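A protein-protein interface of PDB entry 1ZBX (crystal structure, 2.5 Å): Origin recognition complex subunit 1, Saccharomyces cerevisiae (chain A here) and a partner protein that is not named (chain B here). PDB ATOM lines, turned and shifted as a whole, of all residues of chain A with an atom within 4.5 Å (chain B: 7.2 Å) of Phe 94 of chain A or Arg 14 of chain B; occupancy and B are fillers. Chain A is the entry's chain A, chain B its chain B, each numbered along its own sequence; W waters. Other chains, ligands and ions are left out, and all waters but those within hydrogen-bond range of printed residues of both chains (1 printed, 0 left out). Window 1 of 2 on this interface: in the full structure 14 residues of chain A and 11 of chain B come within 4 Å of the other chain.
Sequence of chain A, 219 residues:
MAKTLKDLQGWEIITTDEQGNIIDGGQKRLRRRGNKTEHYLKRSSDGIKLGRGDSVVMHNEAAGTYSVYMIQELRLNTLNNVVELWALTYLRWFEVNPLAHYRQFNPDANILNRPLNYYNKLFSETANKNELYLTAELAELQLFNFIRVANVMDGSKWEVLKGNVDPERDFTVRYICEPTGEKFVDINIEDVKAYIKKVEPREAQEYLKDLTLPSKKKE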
ATOM      1  N   ALA A  63      17.163  -1.409   1.902  1.00  0.00           N
ATOM      2  CA  ALA A  63      16.092  -1.927   2.741  1.00  0.00           C
ATOM      3  C   ALA A  63      15.832  -3.420   2.567  1.00  0.00           C
ATOM      4  O   ALA A  63      15.295  -4.075   3.461  1.00  0.00           O
ATOM      5  CB  ALA A  63      14.818  -1.146   2.481  1.00  0.00           C
ATOM      6  N   GLY A  64      16.203  -3.957   1.411  1.00  0.00           N
ATOM      7  CA  GLY A  64      15.989  -5.370   1.173  1.00  0.00           C
ATOM      8  C   GLY A  64      14.529  -5.701   0.959  1.00  0.00           C
ATOM      9  O   GLY A  64      14.107  -6.833   1.158  1.00  0.00           O
ATOM     10  N   THR A  65      13.754  -4.704   0.556  1.00  0.00           N
ATOM     11  CA  THR A  65      12.330  -4.864   0.292  1.00  0.00           C
ATOM     12  C   THR A  65      11.890  -3.620  -0.472  1.00  0.00           C
ATOM     13  O   THR A  65      12.626  -2.637  -0.501  1.00  0.00           O
ATOM     14  CB  THR A  65      11.522  -5.000   1.606  1.00  0.00           C
ATOM     15  OG1 THR A  65      10.138  -5.176   1.287  1.00  0.00           O
ATOM     16  CG2 THR A  65      11.687  -3.775   2.488  1.00  0.00           C
ATOM     17  N   ARG A  92       5.776   2.219   4.846  1.00  0.00           N
ATOM     18  CA  ARG A  92       4.969   0.994   4.880  1.00  0.00           C
ATOM     19  C   ARG A  92       4.737   0.694   6.359  1.00  0.00           C
ATOM     20  O   ARG A  92       5.452   1.210   7.218  1.00  0.00           O
ATOM     21  CB  ARG A  92       5.682  -0.164   4.193  1.00  0.00           C
ATOM     22  CG  ARG A  92       5.789   0.008   2.696  1.00  0.00           C
ATOM     23  CD  ARG A  92       6.713  -1.018   2.073  1.00  0.00           C
ATOM     24  NE  ARG A  92       6.283  -2.385   2.337  1.00  0.00           N
ATOM     25  CZ  ARG A  92       6.980  -3.460   1.984  1.00  0.00           C
ATOM     26  NH1 ARG A  92       8.143  -3.327   1.353  1.00  0.00           N
ATOM     27  NH2 ARG A  92       6.513  -4.668   2.261  1.00  0.00           N
ATOM     28  N   TRP A  93       3.739  -0.125   6.660  1.00  0.00           N
ATOM     29  CA  TRP A  93       3.412  -0.428   8.049  1.00  0.00           C
ATOM     30  C   TRP A  93       4.597  -0.572   9.017  1.00  0.00           C
ATOM     31  O   TRP A  93       4.609   0.056  10.079  1.00  0.00           O
ATOM     32  CB  TRP A  93       2.542  -1.687   8.122  1.00  0.00           C
ATOM     33  CG  TRP A  93       3.235  -2.891   7.632  1.00  0.00           C
ATOM     34  CD1 TRP A  93       3.450  -3.251   6.330  1.00  0.00           C
ATOM     35  CD2 TRP A  93       3.883  -3.874   8.432  1.00  0.00           C
ATOM     36  NE1 TRP A  93       4.199  -4.401   6.271  1.00  0.00           N
ATOM     37  CE2 TRP A  93       4.479  -4.809   7.548  1.00  0.00           C
ATOM     38  CE3 TRP A  93       4.021  -4.060   9.813  1.00  0.00           C
ATOM     39  CZ2 TRP A  93       5.200  -5.914   7.998  1.00  0.00           C
ATOM     40  CZ3 TRP A  93       4.742  -5.161  10.266  1.00  0.00           C
ATOM     41  CH2 TRP A  93       5.323  -6.077   9.355  1.00  0.00           C
ATOM     42  N   PHE A  94       5.592  -1.376   8.656  1.00  0.00           N
ATOM     43  CA  PHE A  94       6.746  -1.614   9.527  1.00  0.00           C
ATOM     44  C   PHE A  94       7.677  -0.424   9.814  1.00  0.00           C
ATOM     45  O   PHE A  94       8.643  -0.567  10.562  1.00  0.00           O
ATOM     46  CB  PHE A  94       7.570  -2.777   8.974  1.00  0.00           C
ATOM     47  CG  PHE A  94       8.302  -2.452   7.704  1.00  0.00           C
ATOM     48  CD1 PHE A  94       9.552  -1.840   7.741  1.00  0.00           C
ATOM     49  CD2 PHE A  94       7.742  -2.759   6.470  1.00  0.00           C
ATOM     50  CE1 PHE A  94      10.233  -1.544   6.565  1.00  0.00           C
ATOM     51  CE2 PHE A  94       8.408  -2.468   5.291  1.00  0.00           C
ATOM     52  CZ  PHE A  94       9.656  -1.861   5.330  1.00  0.00           C
ATOM     53  N   GLU A  95       7.403   0.740   9.230  1.00  0.00           N
ATOM     54  CA  GLU A  95       8.239   1.908   9.479  1.00  0.00           C
ATOM     55  C   GLU A  95       7.514   2.879  10.391  1.00  0.00           C
ATOM     56  O   GLU A  95       7.986   3.975  10.649  1.00  0.00           O
ATOM     57  CB  GLU A  95       8.603   2.605   8.177  1.00  0.00           C
ATOM     58  CG  GLU A  95       9.174   1.670   7.128  1.00  0.00           C
ATOM     59  CD  GLU A  95       9.571   2.393   5.853  1.00  0.00           C
ATOM     60  OE1 GLU A  95      10.748   2.794   5.739  1.00  0.00           O
ATOM     61  OE2 GLU A  95       8.697   2.568   4.973  1.00  0.00           O
ATOM     62  N   VAL A  96       6.350   2.468  10.870  1.00  0.00           N
ATOM     63  CA  VAL A  96       5.556   3.285  11.780  1.00  0.00           C
ATOM     64  C   VAL A  96       6.089   3.067  13.194  1.00  0.00           C
ATOM     65  O   VAL A  96       6.463   1.949  13.556  1.00  0.00           O
ATOM     66  CB  VAL A  96       4.075   2.843  11.766  1.00  0.00           C
ATOM     67  CG1 VAL A  96       3.327   3.435  12.952  1.00  0.00           C
ATOM     68  CG2 VAL A  96       3.430   3.241  10.472  1.00  0.00           C
ATOM     69  N   TYR B  10       8.868 -10.697  18.390  1.00  0.00           N
ATOM     70  CA  TYR B  10       9.054  -9.628  17.410  1.00  0.00           C
ATOM     71  C   TYR B  10      10.240  -8.757  17.754  1.00  0.00           C
ATOM     72  O   TYR B  10      10.140  -7.873  18.595  1.00  0.00           O
ATOM     73  CB  TYR B  10       7.816  -8.736  17.322  1.00  0.00           C
ATOM     74  CG  TYR B  10       6.699  -9.306  16.488  1.00  0.00           C
ATOM     75  CD1 TYR B  10       5.881 -10.311  16.983  1.00  0.00           C
ATOM     76  CD2 TYR B  10       6.464  -8.840  15.199  1.00  0.00           C
ATOM     77  CE1 TYR B  10       4.849 -10.842  16.217  1.00  0.00           C
ATOM     78  CE2 TYR B  10       5.439  -9.360  14.422  1.00  0.00           C
ATOM     79  CZ  TYR B  10       4.631 -10.362  14.934  1.00  0.00           C
ATOM     80  OH  TYR B  10       3.603 -10.891  14.176  1.00  0.00           O
ATOM     81  N   VAL B  11      11.363  -8.998  17.099  1.00  0.00           N
ATOM     82  CA  VAL B  11      12.561  -8.219  17.340  1.00  0.00           C
ATOM     83  C   VAL B  11      12.334  -6.778  16.921  1.00  0.00           C
ATOM     84  O   VAL B  11      13.033  -5.876  17.355  1.00  0.00           O
ATOM     85  CB  VAL B  11      13.724  -8.788  16.553  1.00  0.00           C
ATOM     86  CG1 VAL B  11      14.941  -7.918  16.726  1.00  0.00           C
ATOM     87  CG2 VAL B  11      14.001 -10.203  17.023  1.00  0.00           C
ATOM     88  N   SER B  12      11.350  -6.581  16.056  1.00  0.00           N
ATOM     89  CA  SER B  12      10.971  -5.263  15.559  1.00  0.00           C
ATOM     90  C   SER B  12       9.643  -5.498  14.838  1.00  0.00           C
ATOM     91  O   SER B  12       9.177  -6.638  14.743  1.00  0.00           O
ATOM     92  CB  SER B  12      12.020  -4.723  14.582  1.00  0.00           C
ATOM     93  OG  SER B  12      11.768  -5.175  13.263  1.00  0.00           O
ATOM     94  N   PRO B  13       9.004  -4.433  14.335  1.00  0.00           N
ATOM     95  CA  PRO B  13       7.725  -4.633  13.638  1.00  0.00           C
ATOM     96  C   PRO B  13       7.888  -5.456  12.362  1.00  0.00           C
ATOM     97  O   PRO B  13       6.987  -6.191  11.960  1.00  0.00           O
ATOM     98  CB  PRO B  13       7.270  -3.209  13.333  1.00  0.00           C
ATOM     99  CG  PRO B  13       7.926  -2.391  14.417  1.00  0.00           C
ATOM    100  CD  PRO B  13       9.299  -2.999  14.502  1.00  0.00           C
ATOM    101  N   ARG B  14       9.052  -5.328  11.735  1.00  0.00           N
ATOM    102  CA  ARG B  14       9.340  -6.034  10.494  1.00  0.00           C
ATOM    103  C   ARG B  14       9.896  -7.444  10.676  1.00  0.00           C
ATOM    104  O   ARG B  14       9.514  -8.368   9.957  1.00  0.00           O
ATOM    105  CB  ARG B  14      10.327  -5.220   9.653  1.00  0.00           C
ATOM    106  CG  ARG B  14      10.852  -5.969   8.446  1.00  0.00           C
ATOM    107  CD  ARG B  14      11.821  -5.118   7.651  1.00  0.00           C
ATOM    108  NE  ARG B  14      12.319  -5.808   6.467  1.00  0.00           N
ATOM    109  CZ  ARG B  14      13.166  -5.268   5.602  1.00  0.00           C
ATOM    110  NH1 ARG B  14      13.609  -4.035   5.801  1.00  0.00           N
ATOM    111  NH2 ARG B  14      13.552  -5.943   4.528  1.00  0.00           N
ATOM    112  N   PHE B  15      10.799  -7.596  11.637  1.00  0.00           N
ATOM    113  CA  PHE B  15      11.435  -8.878  11.893  1.00  0.00           C
ATOM    114  C   PHE B  15      10.868  -9.659  13.065  1.00  0.00           C
ATOM    115  O   PHE B  15      10.772  -9.170  14.183  1.00  0.00           O
ATOM    116  CB  PHE B  15      12.945  -8.676  12.042  1.00  0.00           C
ATOM    117  CG  PHE B  15      13.607  -8.211  10.776  1.00  0.00           C
ATOM    118  CD1 PHE B  15      14.053  -6.901  10.643  1.00  0.00           C
ATOM    119  CD2 PHE B  15      13.725  -9.073   9.682  1.00  0.00           C
ATOM    120  CE1 PHE B  15      14.606  -6.450   9.434  1.00  0.00           C
ATOM    121  CE2 PHE B  15      14.274  -8.635   8.471  1.00  0.00           C
ATOM    122  CZ  PHE B  15      14.715  -7.318   8.347  1.00  0.00           C
ATOM    123  N   LEU B  16      10.499 -10.898  12.774  1.00  0.00           N
ATOM    124  CA  LEU B  16       9.904 -11.822  13.733  1.00  0.00           C
ATOM    125  C   LEU B  16      10.742 -13.096  13.839  1.00  0.00           C
ATOM    126  O   LEU B  16      11.065 -13.711  12.827  1.00  0.00           O
ATOM    127  CB  LEU B  16       8.495 -12.172  13.247  1.00  0.00           C
ATOM    128  CG  LEU B  16       7.709 -13.312  13.870  1.00  0.00           C
ATOM    129  CD1 LEU B  16       7.457 -13.015  15.321  1.00  0.00           C
ATOM    130  CD2 LEU B  16       6.404 -13.473  13.135  1.00  0.00           C
ATOM    131  N   LEU B  22      14.576 -16.250  11.251  1.00  0.00           N
ATOM    132  CA  LEU B  22      14.364 -14.814  11.380  1.00  0.00           C
ATOM    133  C   LEU B  22      13.433 -14.532  10.202  1.00  0.00           C
ATOM    134  O   LEU B  22      13.809 -14.715   9.046  1.00  0.00           O
ATOM    135  CB  LEU B  22      15.684 -14.041  11.216  1.00  0.00           C
ATOM    136  CG  LEU B  22      15.627 -12.504  11.233  1.00  0.00           C
ATOM    137  CD1 LEU B  22      14.891 -12.004  12.486  1.00  0.00           C
ATOM    138  CD2 LEU B  22      17.041 -11.949  11.195  1.00  0.00           C
ATOM    139  N   ILE B  23      12.208 -14.114  10.488  1.00  0.00           N
ATOM    140  CA  ILE B  23      11.265 -13.859   9.415  1.00  0.00           C
ATOM    141  C   ILE B  23      11.089 -12.385   9.081  1.00  0.00           C
ATOM    142  O   ILE B  23      10.698 -11.581   9.921  1.00  0.00           O
ATOM    143  CB  ILE B  23       9.910 -14.489   9.745  1.00  0.00           C
ATOM    144  CG1 ILE B  23      10.090 -15.996   9.882  1.00  0.00           C
ATOM    145  CG2 ILE B  23       8.901 -14.175   8.658  1.00  0.00           C
ATOM    146  CD1 ILE B  23       8.853 -16.724  10.364  1.00  0.00           C
ATOM    147  N   ASP B  24      11.401 -12.049   7.834  1.00  0.00           N
ATOM    148  CA  ASP B  24      11.285 -10.696   7.315  1.00  0.00           C
ATOM    149  C   ASP B  24       9.834 -10.516   6.860  1.00  0.00           C
ATOM    150  O   ASP B  24       9.463 -10.912   5.755  1.00  0.00           O
ATOM    151  CB  ASP B  24      12.232 -10.542   6.130  1.00  0.00           C
ATOM    152  CG  ASP B  24      12.215  -9.157   5.534  1.00  0.00           C
ATOM    153  OD1 ASP B  24      11.150  -8.496   5.575  1.00  0.00           O
ATOM    154  OD2 ASP B  24      13.272  -8.747   5.005  1.00  0.00           O
ATOM    155  N   LEU B  25       9.017  -9.919   7.719  1.00  0.00           N
ATOM    156  CA  LEU B  25       7.611  -9.712   7.404  1.00  0.00           C
ATOM    157  C   LEU B  25       7.371  -8.765   6.236  1.00  0.00           C
ATOM    158  O   LEU B  25       6.320  -8.818   5.615  1.00  0.00           O
ATOM    159  CB  LEU B  25       6.869  -9.217   8.649  1.00  0.00           C
ATOM    160  CG  LEU B  25       6.792 -10.246   9.778  1.00  0.00           C
ATOM    161  CD1 LEU B  25       6.308  -9.590  11.058  1.00  0.00           C
ATOM    162  CD2 LEU B  25       5.872 -11.390   9.355  1.00  0.00           C
ATOM    163  N   ALA B  26       8.341  -7.912   5.926  1.00  0.00           N
ATOM    164  CA  ALA B  26       8.182  -6.970   4.821  1.00  0.00           C
ATOM    165  C   ALA B  26       8.270  -7.698   3.483  1.00  0.00           C
ATOM    166  O   ALA B  26       7.719  -7.246   2.476  1.00  0.00           O
ATOM    167  CB  ALA B  26       9.251  -5.880   4.893  1.00  0.00           C
ATOM    168  N   GLU B  27       8.960  -8.836   3.488  1.00  0.00           N
ATOM    169  CA  GLU B  27       9.146  -9.643   2.291  1.00  0.00           C
ATOM    170  C   GLU B  27       8.375 -10.959   2.342  1.00  0.00           C
ATOM    171  O   GLU B  27       8.281 -11.666   1.339  1.00  0.00           O
ATOM    172  CB  GLU B  27      10.641  -9.921   2.094  1.00  0.00           C
ATOM    173  CG  GLU B  27      11.397  -8.767   1.465  1.00  0.00           C
ATOM    174  CD  GLU B  27      10.932  -8.517   0.049  1.00  0.00           C
ATOM    175  OE1 GLU B  27      11.113  -9.428  -0.784  1.00  0.00           O
ATOM    176  OE2 GLU B  27      10.381  -7.430  -0.232  1.00  0.00           O
ATOM    177  N   ILE B  31      14.935 -14.937   6.313  1.00  0.00           N
ATOM    178  CA  ILE B  31      16.145 -14.229   5.907  1.00  0.00           C
ATOM    179  C   ILE B  31      17.341 -14.816   6.666  1.00  0.00           C
ATOM    180  O   ILE B  31      17.227 -15.158   7.845  1.00  0.00           O
ATOM    181  CB  ILE B  31      16.025 -12.707   6.194  1.00  0.00           C
ATOM    182  CG1 ILE B  31      17.064 -11.936   5.396  1.00  0.00           C
ATOM    183  CG2 ILE B  31      16.231 -12.424   7.665  1.00  0.00           C
ATOM    184  CD1 ILE B  31      17.007 -10.441   5.625  1.00  0.00           C
ATOM    185  N   ARG B  37      22.995  -6.854   5.716  1.00  0.00           N
ATOM    186  CA  ARG B  37      22.010  -5.781   5.796  1.00  0.00           C
ATOM    187  C   ARG B  37      21.539  -5.539   7.223  1.00  0.00           C
ATOM    188  O   ARG B  37      21.354  -4.391   7.637  1.00  0.00           O
ATOM    189  CB  ARG B  37      20.788  -6.090   4.938  1.00  0.00           C
ATOM    190  CG  ARG B  37      20.918  -5.765   3.482  1.00  0.00           C
ATOM    191  CD  ARG B  37      19.552  -5.391   2.966  1.00  0.00           C
ATOM    192  NE  ARG B  37      19.394  -5.651   1.543  1.00  0.00           N
ATOM    193  CZ  ARG B  37      19.461  -6.861   1.000  1.00  0.00           C
ATOM    194  NH1 ARG B  37      19.694  -7.918   1.766  1.00  0.00           N
ATOM    195  NH2 ARG B  37      19.267  -7.013  -0.300  1.00  0.00           N
ATOM    196  N   LEU B  41      20.130  -2.445   9.201  1.00  0.00           N
ATOM    197  CA  LEU B  41      18.689  -2.468   9.413  1.00  0.00           C
ATOM    198  C   LEU B  41      18.250  -2.597  10.864  1.00  0.00           C
ATOM    199  O   LEU B  41      17.156  -2.160  11.217  1.00  0.00           O
ATOM    200  CB  LEU B  41      18.050  -3.596   8.599  1.00  0.00           C
ATOM    201  CG  LEU B  41      18.108  -3.430   7.080  1.00  0.00           C
ATOM    202  CD1 LEU B  41      17.404  -4.585   6.404  1.00  0.00           C
ATOM    203  CD2 LEU B  41      17.464  -2.121   6.695  1.00  0.00           C
ATOM    204  N   LEU B  42      19.091  -3.190  11.707  1.00  0.00           N
ATOM    205  CA  LEU B  42      18.741  -3.375  13.116  1.00  0.00           C
ATOM    206  C   LEU B  42      19.672  -2.686  14.109  1.00  0.00           C
ATOM    207  O   LEU B  42      20.855  -2.481  13.839  1.00  0.00           O
ATOM    208  CB  LEU B  42      18.681  -4.865  13.453  1.00  0.00           C
ATOM    209  CG  LEU B  42      17.510  -5.678  12.909  1.00  0.00           C
ATOM    210  CD1 LEU B  42      17.763  -7.153  13.155  1.00  0.00           C
ATOM    211  CD2 LEU B  42      16.216  -5.237  13.579  1.00  0.00           C
HETATM  212  O   HOH W   1       9.975  -2.952  11.691  1.00  0.00           O
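Water W1 lies within hydrogen-bond range of the backbone NH of Arg 14 of chain B (2.5 Å), the backbone carbonyl oxygen of Phe 94 of chain A (3.0 Å) and the side-chain hydroxyl of Ser 12 of chain B (3.3 Å).
Phe 94 of chain A touches two residues of chain B. Glu 95 of chain A touches none of the printed residues of chain B. Of chain A, only Ala 63 (2.8 Å), Gly 64 (3.5 Å), Thr 65 (3.5 Å) and Phe 94 (3.7 Å) come within 4 Å of Arg 14 of chain B. Of the printed residues of chain A, Ala 26 of chain B touches Thr 65 (3.4 Å), Arg 92 (2.9 Å) and Phe 94 (3.5 Å). Of the printed residues of chain A, Glu 27 of chain B touches Gly 64 (3.3 Å) and Thr 65 (2.7 Å). The nearest residue of chain A that does not touch Arg 14 of chain B is Trp 93 of chain A (4.2 Å). The nearest printed residue of chain B that does not touch Ala 63 of chain A is Arg 37 of chain B (4.2 Å).
Among the printed residues, merely in contact across the chains: Trp 93 of chain A with Pro 13 of chain B (3.0 Å), Gly 64 of chain A with Glu 27 of chain B (3.3 Å), Gly 64 of chain A with Arg 37 of chain B (3.4 Å), Thr 65 of chain A with Arg 14 of chain B (3.5 Å), Gly 64 of chain A with Arg 14 of chain B (3.5 Å), Phe 94 of chain A with Ala 26 of chain B (3.5 Å), Trp 93 of chain A with Leu 25 of chain B (3.6 Å), Ala 63 of chain A with Leu 41 of chain B (3.7 Å) and Phe 94 of chain A with Arg 14 of chain B (3.7 Å).
Hydrophobic or aromatic side chains of chain A within 4 Å of the printed part of chain B: Trp 93 and Phe 94. Among the printed residues, no Asp or Glu carboxylate lies within 4 Å of a Lys or Arg side-chain nitrogen of the other chain.
The backbone carbonyl oxygen (O) of Ala 63 of chain A is in hydrogen-bond range of the guanidinium group (NH2) of Arg 14 of chain B, at 2.8 Å. O of Ala 26 of chain B is in hydrogen-bond range of OG1 of Thr 65 of chain A (3.4 Å). The guanidinium group of Arg 92 of chain A sits at hydrogen-bond distance from the backbone carbonyl oxygen of Ala 26 of chain B (2.9 Å). The side-chain hydroxyl of Thr 65 of chain A is in hydrogen-bond range of the side-chain carboxylate of Glu 27 of chain B.
The backbone NH (N) of Glu 27 of chain B sits at hydrogen-bond distance from the side-chain carboxylate (OD1) of Asp 24 of chain B, at 3.0 Å. The side-chain carboxylate (OE2) of Glu 95 of chain A sits at hydrogen-bond distance from the backbone NH (N) of Arg 92 of chain A (2.9 Å). O of Arg 14 of chain B sits at hydrogen-bond distance from N of Leu 25 of chain B, 2.8 Å away. The backbone NH (N) of Arg 14 of chain B lies within hydrogen-bond range of the side-chain hydroxyl (OG) of Ser 12 of chain B, 3.1 Å away. The side-chain hydroxyl of Thr 65 of chain A sits at hydrogen-bond distance from the guanidinium group of Arg 92 of chain A. The backbone NH of Ala 26 of chain B lies within hydrogen-bond range of the side-chain carboxylate of Asp 24 of chain B.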
